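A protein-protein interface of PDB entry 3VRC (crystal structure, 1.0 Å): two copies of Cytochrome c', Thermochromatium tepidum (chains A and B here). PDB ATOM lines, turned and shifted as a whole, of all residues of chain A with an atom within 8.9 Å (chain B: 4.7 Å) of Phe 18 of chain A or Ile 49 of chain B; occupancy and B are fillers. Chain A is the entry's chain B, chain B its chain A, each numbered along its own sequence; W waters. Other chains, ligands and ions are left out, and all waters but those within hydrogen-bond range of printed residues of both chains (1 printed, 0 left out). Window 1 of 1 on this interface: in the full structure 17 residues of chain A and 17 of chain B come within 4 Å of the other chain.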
ATOM      1  N   GLU A  10      28.412  -3.070  -6.513  1.00  0.00           N
ATOM      2  CA  GLU A  10      27.115  -3.599  -6.923  1.00  0.00           C
ATOM      3  C   GLU A  10      26.348  -2.603  -7.777  1.00  0.00           C
ATOM      4  O   GLU A  10      25.665  -2.995  -8.720  1.00  0.00           O
ATOM      5  CB  GLU A  10      26.297  -3.979  -5.711  1.00  0.00           C
ATOM      6  CG  GLU A  10      26.847  -5.224  -5.041  1.00  0.00           C
ATOM      7  CD  GLU A  10      26.084  -5.507  -3.809  1.00  0.00           C
ATOM      8  OE1 GLU A  10      25.930  -4.544  -2.971  1.00  0.00           O
ATOM      9  OE2 GLU A  10      25.620  -6.681  -3.671  1.00  0.00           O
ATOM     10  N   THR A  11      26.448  -1.336  -7.449  1.00  0.00           N
ATOM     11  CA  THR A  11      25.676  -0.319  -8.174  1.00  0.00           C
ATOM     12  C   THR A  11      26.220  -0.159  -9.603  1.00  0.00           C
ATOM     13  O   THR A  11      25.431  -0.019 -10.549  1.00  0.00           O
ATOM     14  CB  THR A  11      25.639   0.971  -7.427  1.00  0.00           C
ATOM     15  OG1 THR A  11      25.064   0.754  -6.108  1.00  0.00           O
ATOM     16  CG2 THR A  11      24.778   2.035  -8.125  1.00  0.00           C
ATOM     17  N   ARG A  12      27.554  -0.120  -9.761  1.00  0.00           N
ATOM     18  CA  ARG A  12      28.062   0.023 -11.119  1.00  0.00           C
ATOM     19  C   ARG A  12      27.717  -1.201 -11.918  1.00  0.00           C
ATOM     20  O   ARG A  12      27.327  -1.102 -13.102  1.00  0.00           O
ATOM     21  CB  ARG A  12      29.565   0.376 -11.122  1.00  0.00           C
ATOM     22  CG  ARG A  12      30.527  -0.749 -10.702  1.00  0.00           C
ATOM     23  CD  ARG A  12      31.833  -0.156 -10.186  1.00  0.00           C
ATOM     24  NE  ARG A  12      32.843  -1.168  -9.988  1.00  0.00           N
ATOM     25  CZ  ARG A  12      33.961  -0.979  -9.262  1.00  0.00           C
ATOM     26  NH1 ARG A  12      34.158   0.174  -8.621  1.00  0.00           N
ATOM     27  NH2 ARG A  12      34.887  -1.941  -9.265  1.00  0.00           N
ATOM     28  N   GLN A  13      27.830  -2.405 -11.340  1.00  0.00           N
ATOM     29  CA  GLN A  13      27.453  -3.615 -12.026  1.00  0.00           C
ATOM     30  C   GLN A  13      25.992  -3.566 -12.468  1.00  0.00           C
ATOM     31  O   GLN A  13      25.657  -4.024 -13.563  1.00  0.00           O
ATOM     32  CB  GLN A  13      27.684  -4.853 -11.139  1.00  0.00           C
ATOM     33  CG  GLN A  13      29.194  -5.116 -10.986  1.00  0.00           C
ATOM     34  CD  GLN A  13      29.481  -6.217  -9.975  1.00  0.00           C
ATOM     35  OE1 GLN A  13      28.635  -6.572  -9.130  1.00  0.00           O
ATOM     36  NE2 GLN A  13      30.700  -6.710 -10.000  1.00  0.00           N
ATOM     37  N   ALA A  14      25.109  -3.038 -11.619  1.00  0.00           N
ATOM     38  CA  ALA A  14      23.699  -2.906 -11.970  1.00  0.00           C
ATOM     39  C   ALA A  14      23.538  -2.004 -13.187  1.00  0.00           C
ATOM     40  O   ALA A  14      22.730  -2.291 -14.108  1.00  0.00           O
ATOM     41  CB  ALA A  14      22.897  -2.354 -10.785  1.00  0.00           C
ATOM     42  N   GLY A  15      24.212  -0.857 -13.208  1.00  0.00           N
ATOM     43  CA  GLY A  15      24.087   0.021 -14.365  1.00  0.00           C
ATOM     44  C   GLY A  15      24.539  -0.623 -15.648  1.00  0.00           C
ATOM     45  O   GLY A  15      23.870  -0.517 -16.677  1.00  0.00           O
ATOM     46  N   TYR A  16      25.682  -1.327 -15.606  1.00  0.00           N
ATOM     47  CA  TYR A  16      26.139  -1.999 -16.824  1.00  0.00           C
ATOM     48  C   TYR A  16      25.188  -3.085 -17.260  1.00  0.00           C
ATOM     49  O   TYR A  16      24.898  -3.229 -18.447  1.00  0.00           O
ATOM     50  CB  TYR A  16      27.566  -2.592 -16.598  1.00  0.00           C
ATOM     51  CG  TYR A  16      28.613  -1.593 -16.353  1.00  0.00           C
ATOM     52  CD1 TYR A  16      28.845  -0.521 -17.231  1.00  0.00           C
ATOM     53  CD2 TYR A  16      29.447  -1.715 -15.230  1.00  0.00           C
ATOM     54  CE1 TYR A  16      29.828   0.435 -16.976  1.00  0.00           C
ATOM     55  CE2 TYR A  16      30.424  -0.764 -14.974  1.00  0.00           C
ATOM     56  CZ  TYR A  16      30.596   0.319 -15.809  1.00  0.00           C
ATOM     57  OH  TYR A  16      31.534   1.292 -15.498  1.00  0.00           O
ATOM     58  N   ALA A  17      24.677  -3.911 -16.330  1.00  0.00           N
ATOM     59  CA  ALA A  17      23.776  -4.991 -16.684  1.00  0.00           C
ATOM     60  C   ALA A  17      22.508  -4.420 -17.318  1.00  0.00           C
ATOM     61  O   ALA A  17      21.986  -4.976 -18.276  1.00  0.00           O
ATOM     62  CB  ALA A  17      23.407  -5.772 -15.455  1.00  0.00           C
ATOM     63  N   PHE A  18      22.004  -3.295 -16.775  1.00  0.00           N
ATOM     64  CA  PHE A  18      20.772  -2.787 -17.304  1.00  0.00           C
ATOM     65  C   PHE A  18      20.981  -2.149 -18.667  1.00  0.00           C
ATOM     66  O   PHE A  18      20.114  -2.266 -19.555  1.00  0.00           O
ATOM     67  CB  PHE A  18      20.118  -1.810 -16.277  1.00  0.00           C
ATOM     68  CG  PHE A  18      18.633  -1.800 -16.432  1.00  0.00           C
ATOM     69  CD1 PHE A  18      17.869  -2.862 -15.993  1.00  0.00           C
ATOM     70  CD2 PHE A  18      17.951  -0.743 -17.055  1.00  0.00           C
ATOM     71  CE1 PHE A  18      16.494  -2.910 -16.127  1.00  0.00           C
ATOM     72  CE2 PHE A  18      16.585  -0.783 -17.198  1.00  0.00           C
ATOM     73  CZ  PHE A  18      15.851  -1.863 -16.753  1.00  0.00           C
ATOM     74  N   MET A  19      22.132  -1.501 -18.869  1.00  0.00           N
ATOM     75  CA  MET A  19      22.480  -1.019 -20.237  1.00  0.00           C
ATOM     76  C   MET A  19      22.535  -2.191 -21.175  1.00  0.00           C
ATOM     77  O   MET A  19      22.037  -2.065 -22.306  1.00  0.00           O
ATOM     78  CB  MET A  19      23.787  -0.280 -20.261  1.00  0.00           C
ATOM     79  CG  MET A  19      23.721   1.119 -19.697  1.00  0.00           C
ATOM     80  SD  MET A  19      25.121   2.173 -20.200  1.00  0.00           S
ATOM     81  CE  MET A  19      26.472   1.366 -19.335  1.00  0.00           C
ATOM     82  N   ALA A  20      23.200  -3.264 -20.796  1.00  0.00           N
ATOM     83  CA  ALA A  20      23.350  -4.388 -21.698  1.00  0.00           C
ATOM     84  C   ALA A  20      22.023  -4.978 -22.141  1.00  0.00           C
ATOM     85  O   ALA A  20      21.842  -5.296 -23.298  1.00  0.00           O
ATOM     86  CB  ALA A  20      24.230  -5.439 -21.063  1.00  0.00           C
ATOM     87  N   TRP A  21      21.065  -5.058 -21.198  1.00  0.00           N
ATOM     88  CA  TRP A  21      19.750  -5.594 -21.570  1.00  0.00           C
ATOM     89  C   TRP A  21      19.111  -4.698 -22.640  1.00  0.00           C
ATOM     90  O   TRP A  21      18.552  -5.210 -23.625  1.00  0.00           O
ATOM     91  CB  TRP A  21      18.875  -5.617 -20.316  1.00  0.00           C
ATOM     92  CG  TRP A  21      17.489  -6.090 -20.615  1.00  0.00           C
ATOM     93  CD1 TRP A  21      17.103  -7.188 -21.289  1.00  0.00           C
ATOM     94  CD2 TRP A  21      16.262  -5.431 -20.251  1.00  0.00           C
ATOM     95  NE1 TRP A  21      15.736  -7.264 -21.413  1.00  0.00           N
ATOM     96  CE2 TRP A  21      15.200  -6.210 -20.768  1.00  0.00           C
ATOM     97  CE3 TRP A  21      15.966  -4.268 -19.525  1.00  0.00           C
ATOM     98  CZ2 TRP A  21      13.858  -5.843 -20.585  1.00  0.00           C
ATOM     99  CZ3 TRP A  21      14.640  -3.891 -19.369  1.00  0.00           C
ATOM    100  CH2 TRP A  21      13.615  -4.683 -19.893  1.00  0.00           C
ATOM    101  N   ASN A  22      19.195  -3.408 -22.448  1.00  0.00           N
ATOM    102  CA  ASN A  22      18.599  -2.474 -23.423  1.00  0.00           C
ATOM    103  C   ASN A  22      19.354  -2.459 -24.759  1.00  0.00           C
ATOM    104  O   ASN A  22      18.714  -2.393 -25.811  1.00  0.00           O
ATOM    105  CB  ASN A  22      18.447  -1.121 -22.760  1.00  0.00           C
ATOM    106  CG  ASN A  22      17.254  -1.160 -21.804  1.00  0.00           C
ATOM    107  OD1 ASN A  22      16.110  -1.093 -22.260  1.00  0.00           O
ATOM    108  ND2 ASN A  22      17.498  -1.370 -20.513  1.00  0.00           N
ATOM    109  N   MET A  23      20.683  -2.570 -24.740  1.00  0.00           N
ATOM    110  CA  MET A  23      21.434  -2.740 -25.984  1.00  0.00           C
ATOM    111  C   MET A  23      20.946  -3.953 -26.730  1.00  0.00           C
ATOM    112  O   MET A  23      20.792  -3.884 -27.964  1.00  0.00           O
ATOM    113  CB  MET A  23      22.927  -2.852 -25.707  1.00  0.00           C
ATOM    114  CG  MET A  23      23.570  -1.577 -25.205  1.00  0.00           C
ATOM    115  SD  MET A  23      23.760  -0.295 -26.447  1.00  0.00           S
ATOM    116  CE  MET A  23      25.143  -0.928 -27.386  1.00  0.00           C
ATOM    117  N   GLY A  24      20.694  -5.070 -26.041  1.00  0.00           N
ATOM    118  CA  GLY A  24      20.246  -6.261 -26.703  1.00  0.00           C
ATOM    119  C   GLY A  24      18.919  -6.068 -27.375  1.00  0.00           C
ATOM    120  O   GLY A  24      18.678  -6.631 -28.464  1.00  0.00           O
ATOM    121  N   LYS A  25      18.014  -5.271 -26.790  1.00  0.00           N
ATOM    122  CA  LYS A  25      16.742  -5.015 -27.468  1.00  0.00           C
ATOM    123  C   LYS A  25      16.983  -4.220 -28.733  1.00  0.00           C
ATOM    124  O   LYS A  25      16.280  -4.468 -29.741  1.00  0.00           O
ATOM    125  CB  LYS A  25      15.786  -4.221 -26.516  1.00  0.00           C
ATOM    126  CG  LYS A  25      15.314  -5.042 -25.329  1.00  0.00           C
ATOM    127  CD  LYS A  25      14.244  -4.487 -24.430  1.00  0.00           C
ATOM    128  CE  LYS A  25      14.825  -3.581 -23.461  1.00  0.00           C
ATOM    129  NZ  LYS A  25      13.809  -2.823 -22.690  1.00  0.00           N
ATOM    130  N   ALA A  41      12.753   3.702 -26.150  1.00  0.00           N
ATOM    131  CA  ALA A  41      12.804   3.462 -24.702  1.00  0.00           C
ATOM    132  C   ALA A  41      14.176   2.859 -24.325  1.00  0.00           C
ATOM    133  O   ALA A  41      14.773   3.230 -23.314  1.00  0.00           O
ATOM    134  CB  ALA A  41      11.662   2.536 -24.303  1.00  0.00           C
ATOM    135  N   ALA A  42      14.643   1.894 -25.101  1.00  0.00           N
ATOM    136  CA  ALA A  42      15.920   1.233 -24.826  1.00  0.00           C
ATOM    137  C   ALA A  42      17.077   2.205 -24.958  1.00  0.00           C
ATOM    138  O   ALA A  42      17.990   2.223 -24.116  1.00  0.00           O
ATOM    139  CB  ALA A  42      16.087   0.069 -25.747  1.00  0.00           C
ATOM    140  N   ALA A  43      17.089   2.990 -26.034  1.00  0.00           N
ATOM    141  CA  ALA A  43      18.149   3.976 -26.243  1.00  0.00           C
ATOM    142  C   ALA A  43      18.157   5.012 -25.132  1.00  0.00           C
ATOM    143  O   ALA A  43      19.216   5.467 -24.707  1.00  0.00           O
ATOM    144  CB  ALA A  43      17.970   4.660 -27.583  1.00  0.00           C
ATOM    145  N   ASN A  44      16.956   5.394 -24.645  1.00  0.00           N
ATOM    146  CA  ASN A  44      16.909   6.383 -23.548  1.00  0.00           C
ATOM    147  C   ASN A  44      17.568   5.804 -22.280  1.00  0.00           C
ATOM    148  O   ASN A  44      18.189   6.589 -21.546  1.00  0.00           O
ATOM    149  CB  ASN A  44      15.469   6.777 -23.267  1.00  0.00           C
ATOM    150  CG  ASN A  44      14.892   7.660 -24.353  1.00  0.00           C
ATOM    151  OD1 ASN A  44      15.601   8.130 -25.241  1.00  0.00           O
ATOM    152  ND2 ASN A  44      13.600   7.884 -24.249  1.00  0.00           N
ATOM    153  N   VAL A  45      17.404   4.519 -22.044  1.00  0.00           N
ATOM    154  CA  VAL A  45      18.085   3.907 -20.893  1.00  0.00           C
ATOM    155  C   VAL A  45      19.604   4.028 -21.073  1.00  0.00           C
ATOM    156  O   VAL A  45      20.342   4.393 -20.138  1.00  0.00           O
ATOM    157  CB  VAL A  45      17.696   2.453 -20.701  1.00  0.00           C
ATOM    158  CG1 VAL A  45      18.600   1.816 -19.651  1.00  0.00           C
ATOM    159  CG2 VAL A  45      16.249   2.321 -20.278  1.00  0.00           C
ATOM    160  N   VAL A  46      20.108   3.657 -22.251  1.00  0.00           N
ATOM    161  CA  VAL A  46      21.554   3.670 -22.449  1.00  0.00           C
ATOM    162  C   VAL A  46      22.086   5.045 -22.303  1.00  0.00           C
ATOM    163  O   VAL A  46      23.110   5.270 -21.621  1.00  0.00           O
ATOM    164  CB  VAL A  46      21.913   2.983 -23.802  1.00  0.00           C
ATOM    165  CG1 VAL A  46      23.437   3.036 -24.011  1.00  0.00           C
ATOM    166  CG2 VAL A  46      21.428   1.581 -23.870  1.00  0.00           C
ATOM    167  N   ALA A  48      20.770   7.569 -20.603  1.00  0.00           N
ATOM    168  CA  ALA A  48      20.653   8.049 -19.227  1.00  0.00           C
ATOM    169  C   ALA A  48      21.755   7.399 -18.350  1.00  0.00           C
ATOM    170  O   ALA A  48      22.420   8.114 -17.568  1.00  0.00           O
ATOM    171  CB  ALA A  48      19.274   7.789 -18.650  1.00  0.00           C
ATOM    172  N   ILE A  49      21.894   6.102 -18.427  1.00  0.00           N
ATOM    173  CA  ILE A  49      22.885   5.436 -17.571  1.00  0.00           C
ATOM    174  C   ILE A  49      24.302   5.862 -17.937  1.00  0.00           C
ATOM    175  O   ILE A  49      25.124   6.132 -17.046  1.00  0.00           O
ATOM    176  CB  ILE A  49      22.718   3.941 -17.597  1.00  0.00           C
ATOM    177  CG1 ILE A  49      21.334   3.549 -17.010  1.00  0.00           C
ATOM    178  CG2 ILE A  49      23.886   3.251 -16.846  1.00  0.00           C
ATOM    179  CD1 ILE A  49      21.066   2.073 -16.993  1.00  0.00           C
ATOM    180  N   SER A  52      25.114   9.208 -16.195  1.00  0.00           N
ATOM    181  CA  SER A  52      24.652   9.267 -14.819  1.00  0.00           C
ATOM    182  C   SER A  52      25.740   9.482 -13.831  1.00  0.00           C
ATOM    183  O   SER A  52      25.409   9.536 -12.649  1.00  0.00           O
ATOM    184  CB  SER A  52      23.870   7.964 -14.475  1.00  0.00           C
ATOM    185  OG  SER A  52      24.690   6.832 -14.453  1.00  0.00           O
ATOM    186  N   MET A  54      28.703   7.527 -13.338  1.00  0.00           N
ATOM    187  CA  MET A  54      29.189   6.260 -12.786  1.00  0.00           C
ATOM    188  C   MET A  54      30.631   6.312 -12.289  1.00  0.00           C
ATOM    189  O   MET A  54      31.042   5.434 -11.543  1.00  0.00           O
ATOM    190  CB  MET A  54      29.016   5.166 -13.811  1.00  0.00           C
ATOM    191  CG  MET A  54      27.527   4.828 -14.018  1.00  0.00           C
ATOM    192  SD  MET A  54      27.254   3.562 -15.243  1.00  0.00           S
ATOM    193  CE  MET A  54      28.119   2.184 -14.491  1.00  0.00           C
ATOM    194  N   THR B  11      18.287  -8.964 -13.976  1.00  0.00           N
ATOM    195  CA  THR B  11      18.118  -7.712 -14.726  1.00  0.00           C
ATOM    196  C   THR B  11      17.107  -6.796 -14.055  1.00  0.00           C
ATOM    197  O   THR B  11      17.327  -5.574 -13.973  1.00  0.00           O
ATOM    198  CB  THR B  11      17.729  -8.025 -16.188  1.00  0.00           C
ATOM    199  OG1 THR B  11      18.782  -8.810 -16.762  1.00  0.00           O
ATOM    200  CG2 THR B  11      17.640  -6.702 -17.011  1.00  0.00           C
ATOM    201  N   ALA B  14      18.750  -5.280 -11.123  1.00  0.00           N
ATOM    202  CA  ALA B  14      19.672  -4.240 -11.542  1.00  0.00           C
ATOM    203  C   ALA B  14      18.956  -2.922 -11.808  1.00  0.00           C
ATOM    204  O   ALA B  14      19.407  -1.841 -11.457  1.00  0.00           O
ATOM    205  CB  ALA B  14      20.447  -4.675 -12.778  1.00  0.00           C
ATOM    206  N   GLY B  15      17.811  -2.990 -12.513  1.00  0.00           N
ATOM    207  CA  GLY B  15      17.056  -1.780 -12.805  1.00  0.00           C
ATOM    208  C   GLY B  15      16.616  -1.041 -11.551  1.00  0.00           C
ATOM    209  O   GLY B  15      16.736   0.171 -11.407  1.00  0.00           O
ATOM    210  N   PHE B  18      19.603   0.453  -9.662  1.00  0.00           N
ATOM    211  CA  PHE B  18      20.190   1.623 -10.299  1.00  0.00           C
ATOM    212  C   PHE B  18      19.273   2.818 -10.207  1.00  0.00           C
ATOM    213  O   PHE B  18      19.697   3.971  -9.984  1.00  0.00           O
ATOM    214  CB  PHE B  18      20.612   1.326 -11.745  1.00  0.00           C
ATOM    215  CG  PHE B  18      21.729   2.236 -12.196  1.00  0.00           C
ATOM    216  CD1 PHE B  18      23.030   2.052 -11.707  1.00  0.00           C
ATOM    217  CD2 PHE B  18      21.502   3.285 -13.061  1.00  0.00           C
ATOM    218  CE1 PHE B  18      24.047   2.875 -12.107  1.00  0.00           C
ATOM    219  CE2 PHE B  18      22.523   4.128 -13.434  1.00  0.00           C
ATOM    220  CZ  PHE B  18      23.794   3.958 -12.934  1.00  0.00           C
ATOM    221  N   MET B  19      17.941   2.579 -10.292  1.00  0.00           N
ATOM    222  CA  MET B  19      16.949   3.659  -9.973  1.00  0.00           C
ATOM    223  C   MET B  19      17.148   4.171  -8.614  1.00  0.00           C
ATOM    224  O   MET B  19      17.121   5.387  -8.390  1.00  0.00           O
ATOM    225  CB  MET B  19      15.444   3.280 -10.101  1.00  0.00           C
ATOM    226  CG  MET B  19      15.040   3.128 -11.568  1.00  0.00           C
ATOM    227  SD  MET B  19      13.263   3.055 -11.808  1.00  0.00           S
ATOM    228  CE  MET B  19      12.914   1.486 -11.009  1.00  0.00           C
ATOM    229  N   VAL B  45      17.607   8.965 -15.555  1.00  0.00           N
ATOM    230  CA  VAL B  45      17.730   7.531 -15.297  1.00  0.00           C
ATOM    231  C   VAL B  45      16.419   6.956 -14.760  1.00  0.00           C
ATOM    232  O   VAL B  45      15.997   5.897 -15.199  1.00  0.00           O
ATOM    233  CB  VAL B  45      18.876   7.252 -14.274  1.00  0.00           C
ATOM    234  CG1 VAL B  45      18.836   5.779 -13.912  1.00  0.00           C
ATOM    235  CG2 VAL B  45      20.214   7.626 -14.873  1.00  0.00           C
ATOM    236  N   VAL B  46      15.810   7.621 -13.764  1.00  0.00           N
ATOM    237  CA  VAL B  46      14.597   7.060 -13.159  1.00  0.00           C
ATOM    238  C   VAL B  46      13.505   6.939 -14.243  1.00  0.00           C
ATOM    239  O   VAL B  46      12.854   5.894 -14.352  1.00  0.00           O
ATOM    240  CB  VAL B  46      14.175   7.867 -11.957  1.00  0.00           C
ATOM    241  CG1 VAL B  46      12.874   7.333 -11.357  1.00  0.00           C
ATOM    242  CG2 VAL B  46      15.286   7.889 -10.902  1.00  0.00           C
ATOM    243  N   ALA B  47      13.296   8.003 -15.027  1.00  0.00           N
ATOM    244  CA  ALA B  47      12.294   7.953 -16.068  1.00  0.00           C
ATOM    245  C   ALA B  47      12.599   6.879 -17.097  1.00  0.00           C
ATOM    246  O   ALA B  47      11.693   6.168 -17.549  1.00  0.00           O
ATOM    247  CB  ALA B  47      12.132   9.298 -16.729  1.00  0.00           C
ATOM    248  N   ALA B  48      13.850   6.775 -17.512  1.00  0.00           N
ATOM    249  CA  ALA B  48      14.177   5.812 -18.551  1.00  0.00           C
ATOM    250  C   ALA B  48      13.947   4.386 -18.050  1.00  0.00           C
ATOM    251  O   ALA B  48      13.345   3.547 -18.735  1.00  0.00           O
ATOM    252  CB  ALA B  48      15.591   5.978 -19.093  1.00  0.00           C
ATOM    253  N   ILE B  49      14.451   4.072 -16.851  1.00  0.00           N
ATOM    254  CA  ILE B  49      14.288   2.733 -16.325  1.00  0.00           C
ATOM    255  C   ILE B  49      12.792   2.436 -16.092  1.00  0.00           C
ATOM    256  O   ILE B  49      12.328   1.325 -16.397  1.00  0.00           O
ATOM    257  CB  ILE B  49      15.167   2.507 -15.087  1.00  0.00           C
ATOM    258  CG1 ILE B  49      16.646   2.603 -15.502  1.00  0.00           C
ATOM    259  CG2 ILE B  49      14.832   1.161 -14.454  1.00  0.00           C
ATOM    260  CD1 ILE B  49      17.637   2.397 -14.336  1.00  0.00           C
ATOM    261  N   ALA B  50      12.065   3.389 -15.548  1.00  0.00           N
ATOM    262  CA  ALA B  50      10.643   3.151 -15.303  1.00  0.00           C
ATOM    263  C   ALA B  50       9.844   2.902 -16.579  1.00  0.00           C
ATOM    264  O   ALA B  50       8.726   2.426 -16.484  1.00  0.00           O
ATOM    265  CB  ALA B  50      10.082   4.306 -14.497  1.00  0.00           C
ATOM    266  N   ASN B  51      10.313   3.301 -17.735  1.00  0.00           N
ATOM    267  CA  ASN B  51       9.570   3.191 -19.001  1.00  0.00           C
ATOM    268  C   ASN B  51      10.274   2.095 -19.957  1.00  0.00           C
ATOM    269  O   ASN B  51      10.036   1.929 -21.161  1.00  0.00           O
ATOM    270  CB  ASN B  51       9.314   4.642 -19.465  1.00  0.00           C
ATOM    271  CG  ASN B  51       8.320   5.371 -18.566  1.00  0.00           C
ATOM    272  OD1 ASN B  51       7.153   5.094 -18.624  1.00  0.00           O
ATOM    273  ND2 ASN B  51       8.782   6.296 -17.727  1.00  0.00           N
ATOM    274  N   SER B  52      11.110   1.252 -19.393  1.00  0.00           N
ATOM    275  CA  SER B  52      11.958   0.371 -20.181  1.00  0.00           C
ATOM    276  C   SER B  52      11.351  -0.990 -20.375  1.00  0.00           C
ATOM    277  O   SER B  52      12.038  -1.900 -20.820  1.00  0.00           O
ATOM    278  CB  SER B  52      13.346   0.266 -19.478  1.00  0.00           C
ATOM    279  OG  SER B  52      13.273  -0.404 -18.257  1.00  0.00           O
ATOM    280  N   MET B  54      10.058  -3.184 -18.072  1.00  0.00           N
ATOM    281  CA  MET B  54      10.507  -4.157 -17.064  1.00  0.00           C
ATOM    282  C   MET B  54       9.462  -5.260 -16.775  1.00  0.00           C
ATOM    283  O   MET B  54       9.867  -6.296 -16.254  1.00  0.00           O
ATOM    284  CB  MET B  54      10.894  -3.462 -15.768  1.00  0.00           C
ATOM    285  CG  MET B  54      12.184  -2.637 -15.905  1.00  0.00           C
ATOM    286  SD  MET B  54      12.624  -1.742 -14.409  1.00  0.00           S
ATOM    287  CE  MET B  54      12.964  -3.087 -13.274  1.00  0.00           C
ATOM    288  N   LEU B  57      10.422  -8.720 -17.634  1.00  0.00           N
ATOM    289  CA  LEU B  57      11.390  -9.398 -16.747  1.00  0.00           C
ATOM    290  C   LEU B  57      10.630 -10.279 -15.711  1.00  0.00           C
ATOM    291  O   LEU B  57      11.302 -10.803 -14.811  1.00  0.00           O
ATOM    292  CB  LEU B  57      12.339  -8.400 -16.099  1.00  0.00           C
ATOM    293  CG  LEU B  57      13.145  -7.561 -17.146  1.00  0.00           C
ATOM    294  CD1 LEU B  57      13.856  -6.457 -16.434  1.00  0.00           C
ATOM    295  CD2 LEU B  57      14.056  -8.460 -17.977  1.00  0.00           C
HETATM  296  O   HOH W   1      13.045   4.227 -21.406  1.00  0.00           O
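Of the 26 printed residues of chain A, 13 touch a printed residue of chain B. Along chain A the printed residues that touch a printed residue of chain B span positions 11 to 54. Hydrophobic or aromatic side chains of chain B that line the printed part of chain A: Ala 14, Phe 18, Val 45, Ala 48, Ile 49, Met 54 and Leu 57.
Water W1 lies within hydrogen-bond range of O of Ala 41 of chain A (2.8 Å) and O of Ala 48 of chain B (2.8 Å).
NZ of Lys 25 of chain A is in hydrogen-bond range of O of Ser 52 of chain B (2.7 Å).
Among the printed residues, merely in contact across the chains: Phe 18 of chain A with Ser 52 of chain B (3.3 Å), Trp 21 of chain A with Ser 52 of chain B (3.3 Å), Ser 52 of chain A with Phe 18 of chain B (3.4 Å), Thr 11 of chain A with Phe 18 of chain B (3.4 Å), Phe 18 of chain A with Thr 11 of chain B (3.4 Å), Phe 18 of chain A with Gly 15 of chain B (3.5 Å), Gly 15 of chain A with Phe 18 of chain B (3.5 Å), Val 45 of chain A with Ala 48 of chain B (3.5 Å), Ala 48 of chain A with Val 45 of chain B (3.5 Å), Ala 14 of chain A with Ala 14 of chain B (3.6 Å), Ala 41 of chain A with Asn 51 of chain B (3.6 Å), Asn 44 of chain A with Ala 48 of chain B (3.6 Å), Val 45 of chain A with Ser 52 of chain B (3.6 Å), Trp 21 of chain A with Thr 11 of chain B (3.7 Å), Ser 52 of chain A with Val 45 of chain B (3.7 Å), Trp 21 of chain A with Leu 57 of chain B (3.7 Å), Ile 49 of chain A with Phe 18 of chain B (3.8 Å), Phe 18 of chain A with Ile 49 of chain B (3.8 Å), Phe 18 of chain A with Met 54 of chain B (3.8 Å) and Met 54 of chain A with Phe 18 of chain B (3.98 Å).
Thr 11 of chain A touches Phe 18 of chain B, and with the chains exchanged Phe 18 of chain A touches Thr 11 of chain B. Ala 14 of chain B touches its own counterpart, Ala 14 of chain A. Gly 15 of chain A touches Phe 18 of chain B, and with the chains exchanged Phe 18 of chain A touches Gly 15 of chain B. Phe 18 of chain A touches Ile 49 of chain B, and with the chains exchanged Ile 49 of chain A touches Phe 18 of chain B.
Of chain B, only Thr 11 (3.4 Å), Gly 15 (3.5 Å), Ile 49 (3.8 Å), Ser 52 (3.3 Å) and Met 54 (3.8 Å) come within 4 Å of Phe 18 of chain A. Of chain A, only Phe 18 (3.5 Å) comes within 4 Å of Gly 15 of chain B. Ala 48 of chain B touches two residues of chain A. No residue of chain A comes within 4 Å of Ala 50 of chain B. Of the printed residues of chain A, Phe 18 of chain B touches Thr 11, Gly 15, Ile 49, Ser 52 and Met 54. Printed residues of chain B within 4 Å of Thr 11 of chain A: Phe 18 (3.4 Å). Printed residues of chain B within 4 Å of Ala 14 of chain A: Ala 14. Of the printed residues of chain A, Met 54 of chain B touches Phe 18. Gly 24 of chain A touches none of the printed residues of chain B.
The backbone carbonyl oxygen (O) of Ile 49 of chain A lies within hydrogen-bond range of the side-chain hydroxyl (OG) of Ser 52 of chain A, at 2.7 Å. The side-chain amino group (NZ) of Lys 25 of chain A is in hydrogen-bond range of the side-chain amide oxygen (OD1) of Asn 22 of chain A. The side-chain hydroxyl of Ser 52 of chain B lies within hydrogen-bond range of the backbone carbonyl oxygen of Ile 49 of chain B, at 2.7 Å. The backbone carbonyl oxygen of Phe 18 of chain A sits at hydrogen-bond distance from the side-chain amide nitrogen of Asn 22 of chain A. The backbone carbonyl oxygen of Ala 47 of chain B is in hydrogen-bond range of the side-chain amide nitrogen of Asn 51 of chain B, at 2.9 Å.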
